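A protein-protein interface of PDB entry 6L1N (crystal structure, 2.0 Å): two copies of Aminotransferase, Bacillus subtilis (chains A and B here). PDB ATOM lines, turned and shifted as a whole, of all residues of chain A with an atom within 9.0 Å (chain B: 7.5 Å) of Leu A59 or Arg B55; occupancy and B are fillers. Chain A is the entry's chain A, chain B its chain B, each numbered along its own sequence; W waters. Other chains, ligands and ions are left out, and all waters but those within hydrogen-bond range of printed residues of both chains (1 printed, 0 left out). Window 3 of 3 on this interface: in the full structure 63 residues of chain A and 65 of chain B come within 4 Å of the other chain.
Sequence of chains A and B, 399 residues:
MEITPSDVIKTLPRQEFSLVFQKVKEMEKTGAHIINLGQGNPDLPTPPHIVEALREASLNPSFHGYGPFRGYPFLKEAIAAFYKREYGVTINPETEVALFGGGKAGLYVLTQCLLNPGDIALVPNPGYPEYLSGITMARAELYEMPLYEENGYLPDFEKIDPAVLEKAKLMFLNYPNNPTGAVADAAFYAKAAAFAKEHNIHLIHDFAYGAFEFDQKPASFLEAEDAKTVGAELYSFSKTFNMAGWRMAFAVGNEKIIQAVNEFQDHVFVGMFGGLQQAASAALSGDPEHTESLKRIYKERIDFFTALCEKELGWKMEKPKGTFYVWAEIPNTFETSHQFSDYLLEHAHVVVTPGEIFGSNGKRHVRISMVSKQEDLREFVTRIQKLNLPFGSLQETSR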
ATOM      1  N   VAL A  51     -17.448  32.841 -29.278  1.00  0.00           N
ATOM      2  CA  VAL A  51     -18.060  32.019 -28.281  1.00  0.00           C
ATOM      3  C   VAL A  51     -18.851  30.848 -28.924  1.00  0.00           C
ATOM      4  O   VAL A  51     -18.829  29.688 -28.412  1.00  0.00           O
ATOM      5  CB  VAL A  51     -19.001  32.807 -27.384  1.00  0.00           C
ATOM      6  CG1 VAL A  51     -19.651  31.883 -26.387  1.00  0.00           C
ATOM      7  CG2 VAL A  51     -18.272  33.939 -26.655  1.00  0.00           C
ATOM      8  N   GLU A  52     -19.522  31.130 -30.043  1.00  0.00           N
ATOM      9  CA  GLU A  52     -20.413  30.121 -30.639  1.00  0.00           C
ATOM     10  C   GLU A  52     -19.537  29.072 -31.335  1.00  0.00           C
ATOM     11  O   GLU A  52     -19.913  27.906 -31.415  1.00  0.00           O
ATOM     12  CB  GLU A  52     -21.402  30.756 -31.633  1.00  0.00           C
ATOM     13  N   ALA A  53     -18.404  29.491 -31.888  1.00  0.00           N
ATOM     14  CA  ALA A  53     -17.450  28.587 -32.526  1.00  0.00           C
ATOM     15  C   ALA A  53     -16.917  27.607 -31.494  1.00  0.00           C
ATOM     16  O   ALA A  53     -16.834  26.422 -31.800  1.00  0.00           O
ATOM     17  CB  ALA A  53     -16.315  29.331 -33.184  1.00  0.00           C
ATOM     18  N   LEU A  54     -16.574  28.104 -30.292  1.00  0.00           N
ATOM     19  CA  LEU A  54     -16.199  27.257 -29.175  1.00  0.00           C
ATOM     20  C   LEU A  54     -17.319  26.295 -28.746  1.00  0.00           C
ATOM     21  O   LEU A  54     -17.079  25.093 -28.552  1.00  0.00           O
ATOM     22  CB  LEU A  54     -15.834  28.071 -27.963  1.00  0.00           C
ATOM     23  CG  LEU A  54     -15.543  27.212 -26.712  1.00  0.00           C
ATOM     24  CD1 LEU A  54     -14.416  26.233 -26.952  1.00  0.00           C
ATOM     25  CD2 LEU A  54     -15.196  28.085 -25.534  1.00  0.00           C
ATOM     26  N   ARG A  55     -18.528  26.827 -28.560  1.00  0.00           N
ATOM     27  CA  ARG A  55     -19.681  25.991 -28.176  1.00  0.00           C
ATOM     28  C   ARG A  55     -19.996  24.872 -29.159  1.00  0.00           C
ATOM     29  O   ARG A  55     -20.216  23.748 -28.724  1.00  0.00           O
ATOM     30  CB  ARG A  55     -20.926  26.826 -27.889  1.00  0.00           C
ATOM     31  CG  ARG A  55     -20.804  27.665 -26.639  1.00  0.00           C
ATOM     32  CD  ARG A  55     -22.002  28.610 -26.439  1.00  0.00           C
ATOM     33  NE  ARG A  55     -23.078  27.890 -25.767  1.00  0.00           N
ATOM     34  CZ  ARG A  55     -24.063  27.234 -26.375  1.00  0.00           C
ATOM     35  NH1 ARG A  55     -24.170  27.255 -27.692  1.00  0.00           N
ATOM     36  NH2 ARG A  55     -24.962  26.566 -25.645  1.00  0.00           N
ATOM     37  N   GLU A  56     -19.951  25.152 -30.458  1.00  0.00           N
ATOM     38  CA  GLU A  56     -20.137  24.153 -31.483  1.00  0.00           C
ATOM     39  C   GLU A  56     -18.964  23.151 -31.530  1.00  0.00           C
ATOM     40  O   GLU A  56     -19.219  21.977 -31.539  1.00  0.00           O
ATOM     41  CB  GLU A  56     -20.331  24.735 -32.885  1.00  0.00           C
ATOM     42  N   ALA A  57     -17.705  23.645 -31.516  1.00  0.00           N
ATOM     43  CA  ALA A  57     -16.524  22.806 -31.523  1.00  0.00           C
ATOM     44  C   ALA A  57     -16.463  21.757 -30.403  1.00  0.00           C
ATOM     45  O   ALA A  57     -16.007  20.633 -30.622  1.00  0.00           O
ATOM     46  CB  ALA A  57     -15.246  23.660 -31.535  1.00  0.00           C
ATOM     47  N   SER A  58     -16.898  22.137 -29.215  1.00  0.00           N
ATOM     48  CA  SER A  58     -16.844  21.313 -28.031  1.00  0.00           C
ATOM     49  C   SER A  58     -17.656  20.038 -28.123  1.00  0.00           C
ATOM     50  O   SER A  58     -17.386  19.060 -27.427  1.00  0.00           O
ATOM     51  CB  SER A  58     -17.233  22.120 -26.816  1.00  0.00           C
ATOM     52  OG  SER A  58     -18.610  22.244 -26.723  1.00  0.00           O
ATOM     53  N   LEU A  59     -18.603  20.027 -29.056  1.00  0.00           N
ATOM     54  CA  LEU A  59     -19.364  18.858 -29.370  1.00  0.00           C
ATOM     55  C   LEU A  59     -18.643  17.886 -30.306  1.00  0.00           C
ATOM     56  O   LEU A  59     -19.078  16.776 -30.421  1.00  0.00           O
ATOM     57  CB  LEU A  59     -20.686  19.284 -29.984  1.00  0.00           C
ATOM     58  CG  LEU A  59     -21.558  20.236 -29.173  1.00  0.00           C
ATOM     59  CD1 LEU A  59     -22.701  20.729 -30.026  1.00  0.00           C
ATOM     60  CD2 LEU A  59     -22.089  19.535 -27.949  1.00  0.00           C
ATOM     61  N   ASN A  60     -17.558  18.289 -30.960  1.00  0.00           N
ATOM     62  CA  ASN A  60     -16.865  17.429 -31.898  1.00  0.00           C
ATOM     63  C   ASN A  60     -15.845  16.531 -31.144  1.00  0.00           C
ATOM     64  O   ASN A  60     -14.860  17.019 -30.616  1.00  0.00           O
ATOM     65  CB  ASN A  60     -16.192  18.237 -33.007  1.00  0.00           C
ATOM     66  CG  ASN A  60     -15.278  17.373 -33.890  1.00  0.00           C
ATOM     67  OD1 ASN A  60     -15.287  16.145 -33.822  1.00  0.00           O
ATOM     68  ND2 ASN A  60     -14.440  18.028 -34.682  1.00  0.00           N
ATOM     69  N   PRO A  61     -16.112  15.209 -31.106  1.00  0.00           N
ATOM     70  CA  PRO A  61     -15.375  14.267 -30.295  1.00  0.00           C
ATOM     71  C   PRO A  61     -13.908  14.126 -30.703  1.00  0.00           C
ATOM     72  O   PRO A  61     -13.119  13.730 -29.878  1.00  0.00           O
ATOM     73  CB  PRO A  61     -16.152  12.951 -30.488  1.00  0.00           C
ATOM     74  CG  PRO A  61     -16.845  13.111 -31.830  1.00  0.00           C
ATOM     75  CD  PRO A  61     -17.203  14.557 -31.873  1.00  0.00           C
ATOM     76  N   SER A  62     -13.559  14.456 -31.951  1.00  0.00           N
ATOM     77  CA  SER A  62     -12.182  14.583 -32.351  1.00  0.00           C
ATOM     78  C   SER A  62     -11.345  15.482 -31.461  1.00  0.00           C
ATOM     79  O   SER A  62     -10.152  15.248 -31.334  1.00  0.00           O
ATOM     80  CB  SER A  62     -12.044  15.107 -33.781  1.00  0.00           C
ATOM     81  OG  SER A  62     -12.238  14.089 -34.714  1.00  0.00           O
ATOM     82  N   PHE A  63     -11.952  16.506 -30.871  1.00  0.00           N
ATOM     83  CA  PHE A  63     -11.209  17.419 -30.027  1.00  0.00           C
ATOM     84  C   PHE A  63     -11.143  16.961 -28.582  1.00  0.00           C
ATOM     85  O   PHE A  63     -10.450  17.545 -27.779  1.00  0.00           O
ATOM     86  CB  PHE A  63     -11.777  18.840 -30.130  1.00  0.00           C
ATOM     87  CG  PHE A  63     -11.764  19.422 -31.501  1.00  0.00           C
ATOM     88  CD1 PHE A  63     -10.732  19.182 -32.383  1.00  0.00           C
ATOM     89  CD2 PHE A  63     -12.797  20.289 -31.913  1.00  0.00           C
ATOM     90  CE1 PHE A  63     -10.721  19.739 -33.648  1.00  0.00           C
ATOM     91  CE2 PHE A  63     -12.787  20.855 -33.186  1.00  0.00           C
ATOM     92  CZ  PHE A  63     -11.780  20.545 -34.071  1.00  0.00           C
ATOM     93  N   HIS A  64     -11.782  15.852 -28.257  1.00  0.00           N
ATOM     94  CA  HIS A  64     -11.834  15.391 -26.869  1.00  0.00           C
ATOM     95  C   HIS A  64     -10.581  14.612 -26.503  1.00  0.00           C
ATOM     96  O   HIS A  64     -10.241  14.583 -25.348  1.00  0.00           O
ATOM     97  CB  HIS A  64     -13.063  14.493 -26.616  1.00  0.00           C
ATOM     98  CG  HIS A  64     -14.365  15.189 -26.754  1.00  0.00           C
ATOM     99  ND1 HIS A  64     -15.576  14.544 -26.576  1.00  0.00           N
ATOM    100  CD2 HIS A  64     -14.661  16.475 -27.069  1.00  0.00           C
ATOM    101  CE1 HIS A  64     -16.551  15.410 -26.755  1.00  0.00           C
ATOM    102  NE2 HIS A  64     -16.025  16.594 -27.017  1.00  0.00           N
ATOM    103  N   PHE A 273      -6.725  22.747 -26.555  1.00  0.00           N
ATOM    104  CA  PHE A 273      -8.065  22.222 -26.805  1.00  0.00           C
ATOM    105  C   PHE A 273      -8.569  22.657 -28.147  1.00  0.00           C
ATOM    106  O   PHE A 273      -8.654  23.874 -28.428  1.00  0.00           O
ATOM    107  CB  PHE A 273      -9.048  22.613 -25.708  1.00  0.00           C
ATOM    108  CG  PHE A 273     -10.423  22.032 -25.877  1.00  0.00           C
ATOM    109  CD1 PHE A 273     -10.593  20.658 -26.143  1.00  0.00           C
ATOM    110  CD2 PHE A 273     -11.576  22.828 -25.718  1.00  0.00           C
ATOM    111  CE1 PHE A 273     -11.857  20.111 -26.281  1.00  0.00           C
ATOM    112  CE2 PHE A 273     -12.845  22.281 -25.866  1.00  0.00           C
ATOM    113  CZ  PHE A 273     -12.989  20.913 -26.143  1.00  0.00           C
ATOM    114  N   GLY A 274      -8.866  21.652 -28.997  1.00  0.00           N
ATOM    115  CA  GLY A 274      -9.343  21.872 -30.339  1.00  0.00           C
ATOM    116  C   GLY A 274     -10.525  22.848 -30.410  1.00  0.00           C
ATOM    117  O   GLY A 274     -10.672  23.571 -31.380  1.00  0.00           O
ATOM    118  N   GLY A 275     -11.341  22.884 -29.365  1.00  0.00           N
ATOM    119  CA  GLY A 275     -12.424  23.825 -29.256  1.00  0.00           C
ATOM    120  C   GLY A 275     -11.935  25.243 -29.218  1.00  0.00           C
ATOM    121  O   GLY A 275     -12.535  26.147 -29.855  1.00  0.00           O
ATOM    122  N   PRO B  45     -15.556   9.438 -26.200  1.00  0.00           N
ATOM    123  CA  PRO B  45     -15.734  10.874 -25.999  1.00  0.00           C
ATOM    124  C   PRO B  45     -15.800  11.301 -24.555  1.00  0.00           C
ATOM    125  O   PRO B  45     -16.083  10.534 -23.679  1.00  0.00           O
ATOM    126  CB  PRO B  45     -17.094  11.168 -26.693  1.00  0.00           C
ATOM    127  CG  PRO B  45     -17.249  10.075 -27.689  1.00  0.00           C
ATOM    128  CD  PRO B  45     -16.571   8.875 -27.095  1.00  0.00           C
ATOM    129  N   PRO B  48     -21.054  13.696 -21.483  1.00  0.00           N
ATOM    130  CA  PRO B  48     -21.903  14.840 -21.862  1.00  0.00           C
ATOM    131  C   PRO B  48     -22.040  15.960 -20.852  1.00  0.00           C
ATOM    132  O   PRO B  48     -22.055  17.099 -21.223  1.00  0.00           O
ATOM    133  CB  PRO B  48     -23.274  14.180 -22.091  1.00  0.00           C
ATOM    134  CG  PRO B  48     -22.971  12.784 -22.454  1.00  0.00           C
ATOM    135  CD  PRO B  48     -21.747  12.405 -21.671  1.00  0.00           C
ATOM    136  N   HIS B  49     -22.154  15.635 -19.582  1.00  0.00           N
ATOM    137  CA  HIS B  49     -22.324  16.654 -18.529  1.00  0.00           C
ATOM    138  C   HIS B  49     -21.073  17.572 -18.389  1.00  0.00           C
ATOM    139  O   HIS B  49     -21.151  18.723 -17.928  1.00  0.00           O
ATOM    140  CB  HIS B  49     -22.687  15.990 -17.176  1.00  0.00           C
ATOM    141  CG  HIS B  49     -21.564  15.193 -16.543  1.00  0.00           C
ATOM    142  ND1 HIS B  49     -21.074  14.018 -17.080  1.00  0.00           N
ATOM    143  CD2 HIS B  49     -20.831  15.418 -15.426  1.00  0.00           C
ATOM    144  CE1 HIS B  49     -20.102  13.550 -16.310  1.00  0.00           C
ATOM    145  NE2 HIS B  49     -19.956  14.362 -15.287  1.00  0.00           N
ATOM    146  N   ILE B  50     -19.923  17.063 -18.808  1.00  0.00           N
ATOM    147  CA  ILE B  50     -18.705  17.862 -18.798  1.00  0.00           C
ATOM    148  C   ILE B  50     -18.728  18.826 -19.972  1.00  0.00           C
ATOM    149  O   ILE B  50     -18.469  20.016 -19.805  1.00  0.00           O
ATOM    150  CB  ILE B  50     -17.445  16.936 -18.870  1.00  0.00           C
ATOM    151  CG1 ILE B  50     -17.419  16.066 -17.598  1.00  0.00           C
ATOM    152  CG2 ILE B  50     -16.209  17.806 -18.989  1.00  0.00           C
ATOM    153  CD1 ILE B  50     -16.433  14.929 -17.577  1.00  0.00           C
ATOM    154  N   VAL B  51     -19.084  18.317 -21.132  1.00  0.00           N
ATOM    155  CA  VAL B  51     -19.188  19.109 -22.348  1.00  0.00           C
ATOM    156  C   VAL B  51     -20.231  20.225 -22.183  1.00  0.00           C
ATOM    157  O   VAL B  51     -20.010  21.359 -22.627  1.00  0.00           O
ATOM    158  CB  VAL B  51     -19.577  18.265 -23.572  1.00  0.00           C
ATOM    159  CG1 VAL B  51     -19.698  19.105 -24.832  1.00  0.00           C
ATOM    160  CG2 VAL B  51     -18.549  17.189 -23.825  1.00  0.00           C
ATOM    161  N   GLU B  52     -21.360  19.890 -21.561  1.00  0.00           N
ATOM    162  CA  GLU B  52     -22.435  20.872 -21.352  1.00  0.00           C
ATOM    163  C   GLU B  52     -22.035  21.970 -20.368  1.00  0.00           C
ATOM    164  O   GLU B  52     -22.397  23.127 -20.570  1.00  0.00           O
ATOM    165  CB  GLU B  52     -23.727  20.209 -20.887  1.00  0.00           C
ATOM    166  CG  GLU B  52     -24.454  19.305 -21.909  1.00  0.00           C
ATOM    167  CD  GLU B  52     -24.416  19.749 -23.407  1.00  0.00           C
ATOM    168  OE1 GLU B  52     -24.536  20.955 -23.710  1.00  0.00           O
ATOM    169  OE2 GLU B  52     -24.301  18.867 -24.309  1.00  0.00           O
ATOM    170  N   ALA B  53     -21.277  21.603 -19.336  1.00  0.00           N
ATOM    171  CA  ALA B  53     -20.732  22.562 -18.370  1.00  0.00           C
ATOM    172  C   ALA B  53     -19.840  23.604 -19.053  1.00  0.00           C
ATOM    173  O   ALA B  53     -19.955  24.827 -18.769  1.00  0.00           O
ATOM    174  CB  ALA B  53     -19.980  21.860 -17.269  1.00  0.00           C
ATOM    175  N   LEU B  54     -18.962  23.141 -19.952  1.00  0.00           N
ATOM    176  CA  LEU B  54     -18.162  24.039 -20.769  1.00  0.00           C
ATOM    177  C   LEU B  54     -19.036  24.967 -21.657  1.00  0.00           C
ATOM    178  O   LEU B  54     -18.845  26.198 -21.705  1.00  0.00           O
ATOM    179  CB  LEU B  54     -17.219  23.265 -21.706  1.00  0.00           C
ATOM    180  CG  LEU B  54     -16.418  24.120 -22.652  1.00  0.00           C
ATOM    181  CD1 LEU B  54     -15.631  25.183 -21.921  1.00  0.00           C
ATOM    182  CD2 LEU B  54     -15.485  23.320 -23.531  1.00  0.00           C
ATOM    183  N   ARG B  55     -19.954  24.357 -22.376  1.00  0.00           N
ATOM    184  CA  ARG B  55     -20.849  25.083 -23.282  1.00  0.00           C
ATOM    185  C   ARG B  55     -21.597  26.216 -22.580  1.00  0.00           C
ATOM    186  O   ARG B  55     -21.643  27.340 -23.098  1.00  0.00           O
ATOM    187  CB  ARG B  55     -21.834  24.134 -23.945  1.00  0.00           C
ATOM    188  CG  ARG B  55     -21.224  23.286 -25.020  1.00  0.00           C
ATOM    189  CD  ARG B  55     -22.179  22.197 -25.519  1.00  0.00           C
ATOM    190  NE  ARG B  55     -23.543  22.678 -25.857  1.00  0.00           N
ATOM    191  CZ  ARG B  55     -23.871  23.304 -26.980  1.00  0.00           C
ATOM    192  NH1 ARG B  55     -22.968  23.537 -27.913  1.00  0.00           N
ATOM    193  NH2 ARG B  55     -25.111  23.682 -27.180  1.00  0.00           N
ATOM    194  N   GLU B  56     -22.156  25.933 -21.429  1.00  0.00           N
ATOM    195  CA  GLU B  56     -22.846  26.939 -20.636  1.00  0.00           C
ATOM    196  C   GLU B  56     -21.897  27.957 -20.011  1.00  0.00           C
ATOM    197  O   GLU B  56     -22.179  29.126 -20.011  1.00  0.00           O
ATOM    198  CB  GLU B  56     -23.606  26.294 -19.489  1.00  0.00           C
ATOM    199  N   ALA B  57     -20.794  27.502 -19.434  1.00  0.00           N
ATOM    200  CA  ALA B  57     -19.837  28.441 -18.848  1.00  0.00           C
ATOM    201  C   ALA B  57     -19.259  29.403 -19.880  1.00  0.00           C
ATOM    202  O   ALA B  57     -18.970  30.520 -19.563  1.00  0.00           O
ATOM    203  CB  ALA B  57     -18.746  27.728 -18.092  1.00  0.00           C
ATOM    204  N   SER B  58     -19.158  28.999 -21.133  1.00  0.00           N
ATOM    205  CA  SER B  58     -18.584  29.850 -22.138  1.00  0.00           C
ATOM    206  C   SER B  58     -19.426  31.117 -22.413  1.00  0.00           C
ATOM    207  O   SER B  58     -18.924  32.078 -23.041  1.00  0.00           O
ATOM    208  CB  SER B  58     -18.347  29.078 -23.427  1.00  0.00           C
ATOM    209  OG  SER B  58     -19.550  28.802 -24.129  1.00  0.00           O
ATOM    210  N   LEU B  59     -20.669  31.106 -21.940  1.00  0.00           N
ATOM    211  CA  LEU B  59     -21.582  32.211 -22.083  1.00  0.00           C
ATOM    212  C   LEU B  59     -21.384  33.238 -20.981  1.00  0.00           C
ATOM    213  O   LEU B  59     -21.888  34.335 -21.108  1.00  0.00           O
ATOM    214  CB  LEU B  59     -23.037  31.693 -22.086  1.00  0.00           C
ATOM    215  CG  LEU B  59     -23.469  30.937 -23.359  1.00  0.00           C
ATOM    216  CD1 LEU B  59     -24.913  30.376 -23.324  1.00  0.00           C
ATOM    217  CD2 LEU B  59     -23.326  31.798 -24.591  1.00  0.00           C
ATOM    218  N   ASN B  60     -20.610  32.905 -19.936  1.00  0.00           N
ATOM    219  CA  ASN B  60     -20.353  33.805 -18.835  1.00  0.00           C
ATOM    220  C   ASN B  60     -19.179  34.778 -19.106  1.00  0.00           C
ATOM    221  O   ASN B  60     -18.002  34.394 -18.908  1.00  0.00           O
ATOM    222  CB  ASN B  60     -20.109  33.028 -17.552  1.00  0.00           C
ATOM    223  CG  ASN B  60     -19.795  33.940 -16.375  1.00  0.00           C
ATOM    224  OD1 ASN B  60     -19.760  35.168 -16.503  1.00  0.00           O
ATOM    225  ND2 ASN B  60     -19.549  33.339 -15.217  1.00  0.00           N
ATOM    226  N   TRP B 246      -8.387  18.244 -23.749  1.00  0.00           N
ATOM    227  CA  TRP B 246      -8.767  19.440 -22.994  1.00  0.00           C
ATOM    228  C   TRP B 246      -7.577  20.121 -22.275  1.00  0.00           C
ATOM    229  O   TRP B 246      -7.639  21.343 -22.067  1.00  0.00           O
ATOM    230  CB  TRP B 246      -9.855  19.127 -21.969  1.00  0.00           C
ATOM    231  CG  TRP B 246     -11.164  18.619 -22.564  1.00  0.00           C
ATOM    232  CD1 TRP B 246     -11.365  17.539 -23.396  1.00  0.00           C
ATOM    233  CD2 TRP B 246     -12.418  19.201 -22.358  1.00  0.00           C
ATOM    234  NE1 TRP B 246     -12.710  17.409 -23.696  1.00  0.00           N
ATOM    235  CE2 TRP B 246     -13.373  18.429 -23.066  1.00  0.00           C
ATOM    236  CE3 TRP B 246     -12.862  20.290 -21.572  1.00  0.00           C
ATOM    237  CZ2 TRP B 246     -14.764  18.730 -23.037  1.00  0.00           C
ATOM    238  CZ3 TRP B 246     -14.260  20.567 -21.556  1.00  0.00           C
ATOM    239  CH2 TRP B 246     -15.170  19.760 -22.242  1.00  0.00           C
ATOM    240  N   GLY B 275     -14.269  28.625 -18.454  1.00  0.00           N
ATOM    241  CA  GLY B 275     -15.080  27.590 -19.005  1.00  0.00           C
ATOM    242  C   GLY B 275     -14.502  26.187 -18.832  1.00  0.00           C
ATOM    243  O   GLY B 275     -15.234  25.273 -18.465  1.00  0.00           O
ATOM    244  N   ALA B 279     -15.923  23.100 -16.455  1.00  0.00           N
ATOM    245  CA  ALA B 279     -16.002  21.750 -16.993  1.00  0.00           C
ATOM    246  C   ALA B 279     -15.329  20.739 -16.078  1.00  0.00           C
ATOM    247  O   ALA B 279     -15.871  19.651 -15.817  1.00  0.00           O
ATOM    248  CB  ALA B 279     -15.394  21.701 -18.355  1.00  0.00           C
HETATM  249  O   HOH W   1      -6.580  23.582 -23.929  1.00  0.00           O
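The backbone carbonyl oxygen (O) of Arg A55 lies within hydrogen-bond range of the side-chain hydroxyl (OG) of Ser A58, 3.0 Å away. OG of Ser B58 sits at hydrogen-bond distance from O of Arg B55, 2.8 Å away. The guanidinium group (NE) of Arg B55 is in salt-bridge range of the side-chain carboxylate (OE1) of Glu B52. The backbone carbonyl oxygen of Ser A58 lies within hydrogen-bond range of a ring nitrogen (NE2) of His A64 (2.8 Å).
Among the printed residues, 15 pairs touch across the chains.
CG1 of Val A51 touches O of Ser B58, 3.4 Å away. Arg A55 touches Leu B59 (NE to CG, 3.9 Å). CB of Ser A58 touches CD2 of Leu B54, 3.9 Å away. OG of Ser A58 touches CG of Arg B55 (3.3 Å). Leu A59 touches Val B51. CD1 of Leu A59 touches NH1 of Arg B55, at 3.5 Å. ND1 of His A64 touches CB of Pro B45, 3.7 Å away. Val B51 touches His A64. O of His A64 touches CD1 of Trp B246, at 3.7 Å. Phe A273 touches Leu B54.
The guanidinium group of Arg B55 is in hydrogen-bond range of the backbone carbonyl oxygen of Arg A55.
Arg B55 touches its own counterpart, Arg A55. Arg A55 touches Ser B58, and with the chains exchanged Ser A58 touches Arg B55. Arg A55 touches Leu B59, and with the chains exchanged Leu A59 touches Arg B55. Leu A59 touches Val B51, but with the chains exchanged Val A51 does not touch Leu B59 (4.1 Å). Positions printed for both chains: 51, 52, 53, 54, 55, 56, 57, 58, 59, 60 and 275. Of the 15 pairs that touch across the chains among the printed residues, 9 have their exchanged pair printed and touching as well.
Water W1 lies within hydrogen-bond range of the backbone NH (N) of Phe A273 (2.8 Å) and the backbone carbonyl oxygen (O) of Trp B246 (3.1 Å).
Arg B55 touches three residues of chain A. Of chain A, only Ser A58 and Phe A273 come within 4 Å of Leu B54. No residue of chain A comes within 4 Å of Glu B56. Printed residues of chain B within 4 Å of Arg A55: Arg B55, Ser B58 and Leu B59. Of the printed residues of chain B, Phe A273 touches Leu B54 (3.7 Å) and Trp B246 (3.8 Å).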
